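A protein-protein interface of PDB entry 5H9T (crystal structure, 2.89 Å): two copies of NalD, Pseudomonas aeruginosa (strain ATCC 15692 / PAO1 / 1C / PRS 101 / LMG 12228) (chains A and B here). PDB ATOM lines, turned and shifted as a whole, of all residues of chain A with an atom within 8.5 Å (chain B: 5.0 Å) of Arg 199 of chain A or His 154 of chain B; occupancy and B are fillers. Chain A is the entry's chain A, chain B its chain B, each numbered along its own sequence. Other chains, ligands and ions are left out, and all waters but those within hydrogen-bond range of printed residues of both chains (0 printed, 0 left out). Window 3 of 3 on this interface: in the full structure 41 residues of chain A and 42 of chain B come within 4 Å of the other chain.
The guanidinium group (NH1) of Arg 199 of chain A sits at hydrogen-bond distance from a ring nitrogen (ND1) of His 154 of chain B, 2.9 Å away.
Among the printed residues, merely in contact across the chains: His 154 of chain A with Arg 199 of chain B, His 192 of chain A with Gly 156 of chain B, His 192 of chain A with Met 157 of chain B, Pro 196 of chain A with Met 157 of chain B, Pro 196 of chain A with Gly 200 of chain B, Pro 196 of chain A with Leu 201 of chain B, Arg 199 of chain A with Gly 200 of chain B, Gly 200 of chain A with Arg 199 of chain B and Gly 200 of chain A with Gly 200 of chain B.
Arg 199 of chain A touches just these residues of chain B: His 154 and Gly 200.
Of chain A, only Arg 199 (2.9 Å) comes within 4 Å of His 154 of chain B.
Of the printed residues of chain B, His 154 of chain A touches Arg 199 (3.7 Å).
Printed residues of chain A within 4 Å of Gly 156 of chain B: His 192.
Of the printed residues of chain A, Gly 200 of chain B touches Pro 196 (3.2 Å), Arg 199 (3.8 Å) and Gly 200 (3.95 Å).
Leu 201 of chain A touches none of the printed residues of chain B.
The nearest residue of chain B that does not touch Arg 199 of chain A is Pro 155 of chain B (4.7 Å).
The nearest residue of chain A that does not touch His 154 of chain B is Glu 195 of chain A (6.9 Å).
His 154 of chain A touches Arg 199 of chain B, and with the chains exchanged Arg 199 of chain A touches His 154 of chain B.
Arg 199 of chain A touches Gly 200 of chain B, and with the chains exchanged Gly 200 of chain A touches Arg 199 of chain B.
Gly 200 of chain A touches its own counterpart, Gly 200 of chain B.
8 positions are printed for both chains.
The backbone NH (N) of His 154 of chain B is in hydrogen-bond range of the backbone carbonyl oxygen (O) of Leu 201 of chain B.
The side-chain carboxylate (OE2) of Glu 195 of chain A lies within salt-bridge range of the guanidinium group (NH2) of Arg 199 of chain A, 3.0 Å away.
ND1 of His 154 of chain A is in hydrogen-bond range of O of Gly 200 of chain A.
The backbone NH (N) of His 154 of chain A sits at hydrogen-bond distance from the backbone carbonyl oxygen (O) of Leu 201 of chain A, 3.4 Å away.
Of the 11 printed residues of chain B, 6 touch a printed residue of chain A.
Among the printed residues, no Asp or Glu carboxylate lies within 4 Å of a Lys or Arg side-chain nitrogen of the other chain.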
ATOM      1  N   TYR A  89      32.370  25.810  -5.494  1.00  0.00           N
ATOM      2  CA  TYR A  89      31.254  25.400  -6.337  1.00  0.00           C
ATOM      3  C   TYR A  89      31.525  25.717  -7.807  1.00  0.00           C
ATOM      4  O   TYR A  89      31.444  24.837  -8.665  1.00  0.00           O
ATOM      5  CB  TYR A  89      29.980  26.096  -5.900  1.00  0.00           C
ATOM      6  CG  TYR A  89      28.800  25.799  -6.777  1.00  0.00           C
ATOM      7  CD1 TYR A  89      28.021  24.687  -6.554  1.00  0.00           C
ATOM      8  CD2 TYR A  89      28.453  26.641  -7.833  1.00  0.00           C
ATOM      9  CE1 TYR A  89      26.928  24.409  -7.356  1.00  0.00           C
ATOM     10  CE2 TYR A  89      27.357  26.368  -8.640  1.00  0.00           C
ATOM     11  CZ  TYR A  89      26.600  25.248  -8.393  1.00  0.00           C
ATOM     12  OH  TYR A  89      25.520  24.965  -9.181  1.00  0.00           O
ATOM     13  N   ARG A 152      29.498  27.307   8.879  1.00  0.00           N
ATOM     14  CA  ARG A 152      28.398  27.121   7.932  1.00  0.00           C
ATOM     15  C   ARG A 152      28.038  25.660   7.695  1.00  0.00           C
ATOM     16  O   ARG A 152      26.986  25.359   7.139  1.00  0.00           O
ATOM     17  CB  ARG A 152      28.724  27.803   6.606  1.00  0.00           C
ATOM     18  CG  ARG A 152      29.050  29.285   6.757  1.00  0.00           C
ATOM     19  CD  ARG A 152      29.430  29.922   5.427  1.00  0.00           C
ATOM     20  NE  ARG A 152      28.330  29.864   4.465  1.00  0.00           N
ATOM     21  CZ  ARG A 152      28.418  30.199   3.174  1.00  0.00           C
ATOM     22  NH1 ARG A 152      29.568  30.630   2.642  1.00  0.00           N
ATOM     23  NH2 ARG A 152      27.341  30.103   2.390  1.00  0.00           N
ATOM     24  N   LEU A 153      28.911  24.748   8.102  1.00  0.00           N
ATOM     25  CA  LEU A 153      28.656  23.320   7.918  1.00  0.00           C
ATOM     26  C   LEU A 153      27.628  22.821   8.911  1.00  0.00           C
ATOM     27  O   LEU A 153      27.534  23.353  10.002  1.00  0.00           O
ATOM     28  CB  LEU A 153      29.930  22.532   8.160  1.00  0.00           C
ATOM     29  CG  LEU A 153      31.111  22.789   7.238  1.00  0.00           C
ATOM     30  CD1 LEU A 153      32.404  22.133   7.690  1.00  0.00           C
ATOM     31  CD2 LEU A 153      30.754  22.287   5.868  1.00  0.00           C
ATOM     32  N   HIS A 154      26.889  21.778   8.543  1.00  0.00           N
ATOM     33  CA  HIS A 154      25.888  21.191   9.451  1.00  0.00           C
ATOM     34  C   HIS A 154      26.563  20.504  10.636  1.00  0.00           C
ATOM     35  O   HIS A 154      27.752  20.186  10.573  1.00  0.00           O
ATOM     36  CB  HIS A 154      24.987  20.188   8.710  1.00  0.00           C
ATOM     37  CG  HIS A 154      23.963  20.826   7.823  1.00  0.00           C
ATOM     38  ND1 HIS A 154      24.234  21.230   6.533  1.00  0.00           N
ATOM     39  CD2 HIS A 154      22.661  21.119   8.041  1.00  0.00           C
ATOM     40  CE1 HIS A 154      23.144  21.755   5.998  1.00  0.00           C
ATOM     41  NE2 HIS A 154      22.175  21.696   6.893  1.00  0.00           N
ATOM     42  N   GLU A 191      24.937  21.860 -12.799  1.00  0.00           N
ATOM     43  CA  GLU A 191      24.511  22.590 -11.631  1.00  0.00           C
ATOM     44  C   GLU A 191      23.592  21.812 -10.751  1.00  0.00           C
ATOM     45  O   GLU A 191      23.631  21.935  -9.558  1.00  0.00           O
ATOM     46  CB  GLU A 191      23.914  23.931 -11.974  1.00  0.00           C
ATOM     47  CG  GLU A 191      23.008  23.978 -13.167  1.00  0.00           C
ATOM     48  CD  GLU A 191      22.501  25.378 -13.378  1.00  0.00           C
ATOM     49  OE1 GLU A 191      23.247  26.314 -13.064  1.00  0.00           O
ATOM     50  OE2 GLU A 191      21.364  25.547 -13.836  1.00  0.00           O
ATOM     51  N   HIS A 192      22.726  21.036 -11.352  1.00  0.00           N
ATOM     52  CA  HIS A 192      21.758  20.233 -10.590  1.00  0.00           C
ATOM     53  C   HIS A 192      22.344  18.973  -9.973  1.00  0.00           C
ATOM     54  O   HIS A 192      21.861  18.505  -8.948  1.00  0.00           O
ATOM     55  CB  HIS A 192      20.591  19.840 -11.483  1.00  0.00           C
ATOM     56  CG  HIS A 192      19.861  21.011 -12.058  1.00  0.00           C
ATOM     57  ND1 HIS A 192      19.223  21.947 -11.271  1.00  0.00           N
ATOM     58  CD2 HIS A 192      19.686  21.409 -13.343  1.00  0.00           C
ATOM     59  CE1 HIS A 192      18.678  22.866 -12.047  1.00  0.00           C
ATOM     60  NE2 HIS A 192      18.946  22.565 -13.307  1.00  0.00           N
ATOM     61  N   LEU A 194      25.485  18.825  -8.842  1.00  0.00           N
ATOM     62  CA  LEU A 194      26.283  19.314  -7.719  1.00  0.00           C
ATOM     63  C   LEU A 194      25.439  19.919  -6.592  1.00  0.00           C
ATOM     64  O   LEU A 194      25.806  19.828  -5.422  1.00  0.00           O
ATOM     65  CB  LEU A 194      27.302  20.350  -8.209  1.00  0.00           C
ATOM     66  CG  LEU A 194      28.367  19.834  -9.176  1.00  0.00           C
ATOM     67  CD1 LEU A 194      29.150  20.999  -9.753  1.00  0.00           C
ATOM     68  CD2 LEU A 194      29.309  18.873  -8.484  1.00  0.00           C
ATOM     69  N   GLU A 195      24.316  20.530  -6.953  1.00  0.00           N
ATOM     70  CA  GLU A 195      23.454  21.211  -5.983  1.00  0.00           C
ATOM     71  C   GLU A 195      23.292  20.453  -4.663  1.00  0.00           C
ATOM     72  O   GLU A 195      23.609  20.988  -3.591  1.00  0.00           O
ATOM     73  CB  GLU A 195      22.072  21.499  -6.594  1.00  0.00           C
ATOM     74  CG  GLU A 195      21.132  22.275  -5.639  1.00  0.00           C
ATOM     75  CD  GLU A 195      21.550  23.723  -5.416  1.00  0.00           C
ATOM     76  OE1 GLU A 195      22.599  24.169  -5.932  1.00  0.00           O
ATOM     77  OE2 GLU A 195      20.817  24.439  -4.705  1.00  0.00           O
ATOM     78  N   PRO A 196      22.789  19.218  -4.723  1.00  0.00           N
ATOM     79  CA  PRO A 196      22.471  18.564  -3.456  1.00  0.00           C
ATOM     80  C   PRO A 196      23.665  18.371  -2.529  1.00  0.00           C
ATOM     81  O   PRO A 196      23.508  18.414  -1.313  1.00  0.00           O
ATOM     82  CB  PRO A 196      21.891  17.210  -3.881  1.00  0.00           C
ATOM     83  CG  PRO A 196      22.377  16.990  -5.260  1.00  0.00           C
ATOM     84  CD  PRO A 196      22.546  18.343  -5.879  1.00  0.00           C
ATOM     85  N   MET A 197      24.846  18.153  -3.086  1.00  0.00           N
ATOM     86  CA  MET A 197      26.019  17.967  -2.234  1.00  0.00           C
ATOM     87  C   MET A 197      26.310  19.253  -1.482  1.00  0.00           C
ATOM     88  O   MET A 197      26.548  19.233  -0.280  1.00  0.00           O
ATOM     89  CB  MET A 197      27.238  17.522  -3.038  1.00  0.00           C
ATOM     90  CG  MET A 197      28.513  17.377  -2.220  1.00  0.00           C
ATOM     91  SD  MET A 197      28.388  16.221  -0.836  1.00  0.00           S
ATOM     92  CE  MET A 197      28.429  14.662  -1.703  1.00  0.00           C
ATOM     93  N   PHE A 198      26.283  20.377  -2.186  1.00  0.00           N
ATOM     94  CA  PHE A 198      26.525  21.670  -1.537  1.00  0.00           C
ATOM     95  C   PHE A 198      25.403  22.070  -0.588  1.00  0.00           C
ATOM     96  O   PHE A 198      25.668  22.608   0.485  1.00  0.00           O
ATOM     97  CB  PHE A 198      26.767  22.759  -2.568  1.00  0.00           C
ATOM     98  CG  PHE A 198      28.144  22.725  -3.125  1.00  0.00           C
ATOM     99  CD1 PHE A 198      28.445  21.905  -4.205  1.00  0.00           C
ATOM    100  CD2 PHE A 198      29.156  23.453  -2.531  1.00  0.00           C
ATOM    101  CE1 PHE A 198      29.723  21.846  -4.710  1.00  0.00           C
ATOM    102  CE2 PHE A 198      30.432  23.405  -3.036  1.00  0.00           C
ATOM    103  CZ  PHE A 198      30.718  22.604  -4.129  1.00  0.00           C
ATOM    104  N   ARG A 199      24.162  21.791  -0.972  1.00  0.00           N
ATOM    105  CA  ARG A 199      23.041  22.041  -0.078  1.00  0.00           C
ATOM    106  C   ARG A 199      23.163  21.193   1.198  1.00  0.00           C
ATOM    107  O   ARG A 199      22.835  21.656   2.284  1.00  0.00           O
ATOM    108  CB  ARG A 199      21.704  21.779  -0.784  1.00  0.00           C
ATOM    109  CG  ARG A 199      20.485  22.075   0.080  1.00  0.00           C
ATOM    110  CD  ARG A 199      19.156  21.883  -0.647  1.00  0.00           C
ATOM    111  NE  ARG A 199      19.050  22.369  -2.035  1.00  0.00           N
ATOM    112  CZ  ARG A 199      18.130  23.219  -2.504  1.00  0.00           C
ATOM    113  NH1 ARG A 199      17.204  23.766  -1.721  1.00  0.00           N
ATOM    114  NH2 ARG A 199      18.149  23.538  -3.792  1.00  0.00           N
ATOM    115  N   GLY A 200      23.623  19.953   1.061  1.00  0.00           N
ATOM    116  CA  GLY A 200      23.761  19.043   2.199  1.00  0.00           C
ATOM    117  C   GLY A 200      24.933  19.334   3.117  1.00  0.00           C
ATOM    118  O   GLY A 200      24.945  18.902   4.270  1.00  0.00           O
ATOM    119  N   LEU A 201      25.943  20.028   2.600  1.00  0.00           N
ATOM    120  CA  LEU A 201      27.149  20.344   3.376  1.00  0.00           C
ATOM    121  C   LEU A 201      27.031  21.678   4.107  1.00  0.00           C
ATOM    122  O   LEU A 201      27.524  21.800   5.233  1.00  0.00           O
ATOM    123  CB  LEU A 201      28.390  20.378   2.480  1.00  0.00           C
ATOM    124  CG  LEU A 201      28.863  19.055   1.887  1.00  0.00           C
ATOM    125  CD1 LEU A 201      29.993  19.308   0.897  1.00  0.00           C
ATOM    126  CD2 LEU A 201      29.315  18.084   2.959  1.00  0.00           C
ATOM    127  N   VAL A 202      26.382  22.657   3.474  1.00  0.00           N
ATOM    128  CA  VAL A 202      26.381  24.048   3.947  1.00  0.00           C
ATOM    129  C   VAL A 202      24.956  24.527   4.264  1.00  0.00           C
ATOM    130  O   VAL A 202      24.031  24.305   3.488  1.00  0.00           O
ATOM    131  CB  VAL A 202      26.992  24.995   2.872  1.00  0.00           C
ATOM    132  CG1 VAL A 202      27.161  26.396   3.430  1.00  0.00           C
ATOM    133  CG2 VAL A 202      28.337  24.502   2.358  1.00  0.00           C
ATOM    134  N   ARG A 203      24.794  25.201   5.402  1.00  0.00           N
ATOM    135  CA  ARG A 203      23.468  25.556   5.918  1.00  0.00           C
ATOM    136  C   ARG A 203      22.661  26.480   5.038  1.00  0.00           C
ATOM    137  O   ARG A 203      21.534  26.167   4.664  1.00  0.00           O
ATOM    138  CB  ARG A 203      23.581  26.213   7.289  1.00  0.00           C
ATOM    139  CG  ARG A 203      23.780  25.246   8.428  1.00  0.00           C
ATOM    140  CD  ARG A 203      23.463  25.937   9.744  1.00  0.00           C
ATOM    141  NE  ARG A 203      24.637  25.956  10.611  1.00  0.00           N
ATOM    142  CZ  ARG A 203      24.953  24.953  11.415  1.00  0.00           C
ATOM    143  NH1 ARG A 203      24.170  23.882  11.459  1.00  0.00           N
ATOM    144  NH2 ARG A 203      26.036  25.021  12.181  1.00  0.00           N
ATOM    145  N   ASP A 204      23.235  27.627   4.721  1.00  0.00           N
ATOM    146  CA  ASP A 204      22.505  28.689   4.060  1.00  0.00           C
ATOM    147  C   ASP A 204      22.560  28.610   2.533  1.00  0.00           C
ATOM    148  O   ASP A 204      22.429  29.628   1.860  1.00  0.00           O
ATOM    149  CB  ASP A 204      23.116  30.024   4.532  1.00  0.00           C
ATOM    150  CG  ASP A 204      24.634  30.072   4.331  1.00  0.00           C
ATOM    151  OD1 ASP A 204      25.305  29.049   4.627  1.00  0.00           O
ATOM    152  OD2 ASP A 204      25.153  31.122   3.872  1.00  0.00           O
ATOM    153  N   TRP A 205      22.748  27.416   1.979  1.00  0.00           N
ATOM    154  CA  TRP A 205      22.945  27.294   0.549  1.00  0.00           C
ATOM    155  C   TRP A 205      21.634  27.599  -0.179  1.00  0.00           C
ATOM    156  O   TRP A 205      21.503  28.638  -0.826  1.00  0.00           O
ATOM    157  CB  TRP A 205      23.461  25.901   0.179  1.00  0.00           C
ATOM    158  CG  TRP A 205      24.035  25.869  -1.183  1.00  0.00           C
ATOM    159  CD1 TRP A 205      23.411  25.459  -2.324  1.00  0.00           C
ATOM    160  CD2 TRP A 205      25.341  26.301  -1.575  1.00  0.00           C
ATOM    161  NE1 TRP A 205      24.250  25.600  -3.403  1.00  0.00           N
ATOM    162  CE2 TRP A 205      25.443  26.109  -2.970  1.00  0.00           C
ATOM    163  CE3 TRP A 205      26.439  26.816  -0.882  1.00  0.00           C
ATOM    164  CZ2 TRP A 205      26.598  26.409  -3.691  1.00  0.00           C
ATOM    165  CZ3 TRP A 205      27.591  27.120  -1.595  1.00  0.00           C
ATOM    166  CH2 TRP A 205      27.661  26.911  -2.989  1.00  0.00           C
ATOM    167  N   ARG B 152       8.857  14.944  -1.695  1.00  0.00           N
ATOM    168  CA  ARG B 152       9.885  15.198  -0.689  1.00  0.00           C
ATOM    169  C   ARG B 152      11.161  15.828  -1.257  1.00  0.00           C
ATOM    170  O   ARG B 152      11.985  16.346  -0.503  1.00  0.00           O
ATOM    171  CB  ARG B 152      10.228  13.910   0.053  1.00  0.00           C
ATOM    172  CG  ARG B 152       9.015  13.239   0.683  1.00  0.00           C
ATOM    173  CD  ARG B 152       9.382  11.930   1.364  1.00  0.00           C
ATOM    174  NE  ARG B 152      10.330  12.136   2.463  1.00  0.00           N
ATOM    175  CZ  ARG B 152      10.959  11.165   3.135  1.00  0.00           C
ATOM    176  NH1 ARG B 152      10.747   9.878   2.847  1.00  0.00           N
ATOM    177  NH2 ARG B 152      11.807  11.477   4.114  1.00  0.00           N
ATOM    178  N   LEU B 153      11.322  15.793  -2.575  1.00  0.00           N
ATOM    179  CA  LEU B 153      12.497  16.377  -3.211  1.00  0.00           C
ATOM    180  C   LEU B 153      12.409  17.889  -3.229  1.00  0.00           C
ATOM    181  O   LEU B 153      11.318  18.434  -3.280  1.00  0.00           O
ATOM    182  CB  LEU B 153      12.591  15.921  -4.647  1.00  0.00           C
ATOM    183  CG  LEU B 153      12.761  14.437  -4.909  1.00  0.00           C
ATOM    184  CD1 LEU B 153      12.614  14.043  -6.374  1.00  0.00           C
ATOM    185  CD2 LEU B 153      14.118  14.026  -4.420  1.00  0.00           C
ATOM    186  N   HIS B 154      13.558  18.561  -3.216  1.00  0.00           N
ATOM    187  CA  HIS B 154      13.582  20.026  -3.261  1.00  0.00           C
ATOM    188  C   HIS B 154      13.106  20.540  -4.621  1.00  0.00           C
ATOM    189  O   HIS B 154      13.098  19.786  -5.599  1.00  0.00           O
ATOM    190  CB  HIS B 154      14.986  20.551  -2.952  1.00  0.00           C
ATOM    191  CG  HIS B 154      15.394  20.366  -1.518  1.00  0.00           C
ATOM    192  ND1 HIS B 154      15.765  21.417  -0.707  1.00  0.00           N
ATOM    193  CD2 HIS B 154      15.490  19.253  -0.752  1.00  0.00           C
ATOM    194  CE1 HIS B 154      16.077  20.960   0.493  1.00  0.00           C
ATOM    195  NE2 HIS B 154      15.916  19.649   0.494  1.00  0.00           N
ATOM    196  N   PRO B 155      12.674  21.816  -4.685  1.00  0.00           N
ATOM    197  CA  PRO B 155      12.308  22.454  -5.952  1.00  0.00           C
ATOM    198  C   PRO B 155      13.407  22.296  -7.010  1.00  0.00           C
ATOM    199  O   PRO B 155      14.580  22.445  -6.690  1.00  0.00           O
ATOM    200  CB  PRO B 155      12.196  23.931  -5.568  1.00  0.00           C
ATOM    201  CG  PRO B 155      11.765  23.902  -4.148  1.00  0.00           C
ATOM    202  CD  PRO B 155      12.488  22.735  -3.547  1.00  0.00           C
ATOM    203  N   GLY B 156      13.032  21.984  -8.248  1.00  0.00           N
ATOM    204  CA  GLY B 156      13.996  21.889  -9.364  1.00  0.00           C
ATOM    205  C   GLY B 156      14.849  20.628  -9.401  1.00  0.00           C
ATOM    206  O   GLY B 156      15.646  20.434 -10.322  1.00  0.00           O
ATOM    207  N   MET B 157      14.696  19.784  -8.387  1.00  0.00           N
ATOM    208  CA  MET B 157      15.382  18.511  -8.308  1.00  0.00           C
ATOM    209  C   MET B 157      14.500  17.379  -8.856  1.00  0.00           C
ATOM    210  O   MET B 157      13.470  17.075  -8.278  1.00  0.00           O
ATOM    211  CB  MET B 157      15.778  18.285  -6.844  1.00  0.00           C
ATOM    212  CG  MET B 157      16.671  17.104  -6.582  1.00  0.00           C
ATOM    213  SD  MET B 157      18.065  17.014  -7.725  1.00  0.00           S
ATOM    214  CE  MET B 157      19.228  18.271  -7.209  1.00  0.00           C
ATOM    215  N   ARG B 199      20.626  14.638   2.485  1.00  0.00           N
ATOM    216  CA  ARG B 199      20.106  15.896   3.032  1.00  0.00           C
ATOM    217  C   ARG B 199      19.813  16.912   1.918  1.00  0.00           C
ATOM    218  O   ARG B 199      18.821  17.627   1.978  1.00  0.00           O
ATOM    219  CB  ARG B 199      21.069  16.493   4.065  1.00  0.00           C
ATOM    220  CG  ARG B 199      20.543  17.766   4.699  1.00  0.00           C
ATOM    221  CD  ARG B 199      21.392  18.254   5.838  1.00  0.00           C
ATOM    222  NE  ARG B 199      21.538  17.209   6.832  1.00  0.00           N
ATOM    223  N   GLY B 200      20.668  16.953   0.900  1.00  0.00           N
ATOM    224  CA  GLY B 200      20.498  17.868  -0.229  1.00  0.00           C
ATOM    225  C   GLY B 200      19.408  17.498  -1.221  1.00  0.00           C
ATOM    226  O   GLY B 200      18.917  18.351  -1.956  1.00  0.00           O
ATOM    227  N   LEU B 201      19.031  16.223  -1.257  1.00  0.00           N
ATOM    228  CA  LEU B 201      17.999  15.738  -2.183  1.00  0.00           C
ATOM    229  C   LEU B 201      16.599  15.779  -1.578  1.00  0.00           C
ATOM    230  O   LEU B 201      15.638  16.082  -2.289  1.00  0.00           O
ATOM    231  CB  LEU B 201      18.297  14.301  -2.634  1.00  0.00           C
ATOM    232  CG  LEU B 201      19.512  14.076  -3.533  1.00  0.00           C
ATOM    233  CD1 LEU B 201      19.737  12.585  -3.728  1.00  0.00           C
ATOM    234  CD2 LEU B 201      19.355  14.772  -4.869  1.00  0.00           C
ATOM    235  N   VAL B 202      16.493  15.485  -0.279  1.00  0.00           N
ATOM    236  CA  VAL B 202      15.200  15.279   0.397  1.00  0.00           C
ATOM    237  C   VAL B 202      14.978  16.300   1.525  1.00  0.00           C
ATOM    238  O   VAL B 202      15.871  16.556   2.327  1.00  0.00           O
ATOM    239  CB  VAL B 202      15.124  13.856   1.010  1.00  0.00           C
ATOM    240  CG1 VAL B 202      13.726  13.572   1.534  1.00  0.00           C
ATOM    241  CG2 VAL B 202      15.512  12.777   0.006  1.00  0.00           C
ATOM    242  N   ARG B 203      13.772  16.851   1.563  1.00  0.00           N
ATOM    243  CA  ARG B 203      13.379  17.944   2.446  1.00  0.00           C
ATOM    244  C   ARG B 203      13.532  17.694   3.934  1.00  0.00           C
ATOM    245  O   ARG B 203      14.191  18.441   4.639  1.00  0.00           O
ATOM    246  CB  ARG B 203      11.914  18.262   2.206  1.00  0.00           C
ATOM    247  CG  ARG B 203      11.591  19.122   0.999  1.00  0.00           C
ATOM    248  CD  ARG B 203      10.085  19.120   0.778  1.00  0.00           C
ATOM    249  NE  ARG B 203       9.630  20.093  -0.203  1.00  0.00           N
ATOM    250  CZ  ARG B 203      10.100  21.328  -0.311  1.00  0.00           C
ATOM    251  NH1 ARG B 203      11.055  21.755   0.497  1.00  0.00           N
ATOM    252  NH2 ARG B 203       9.618  22.137  -1.234  1.00  0.00           N
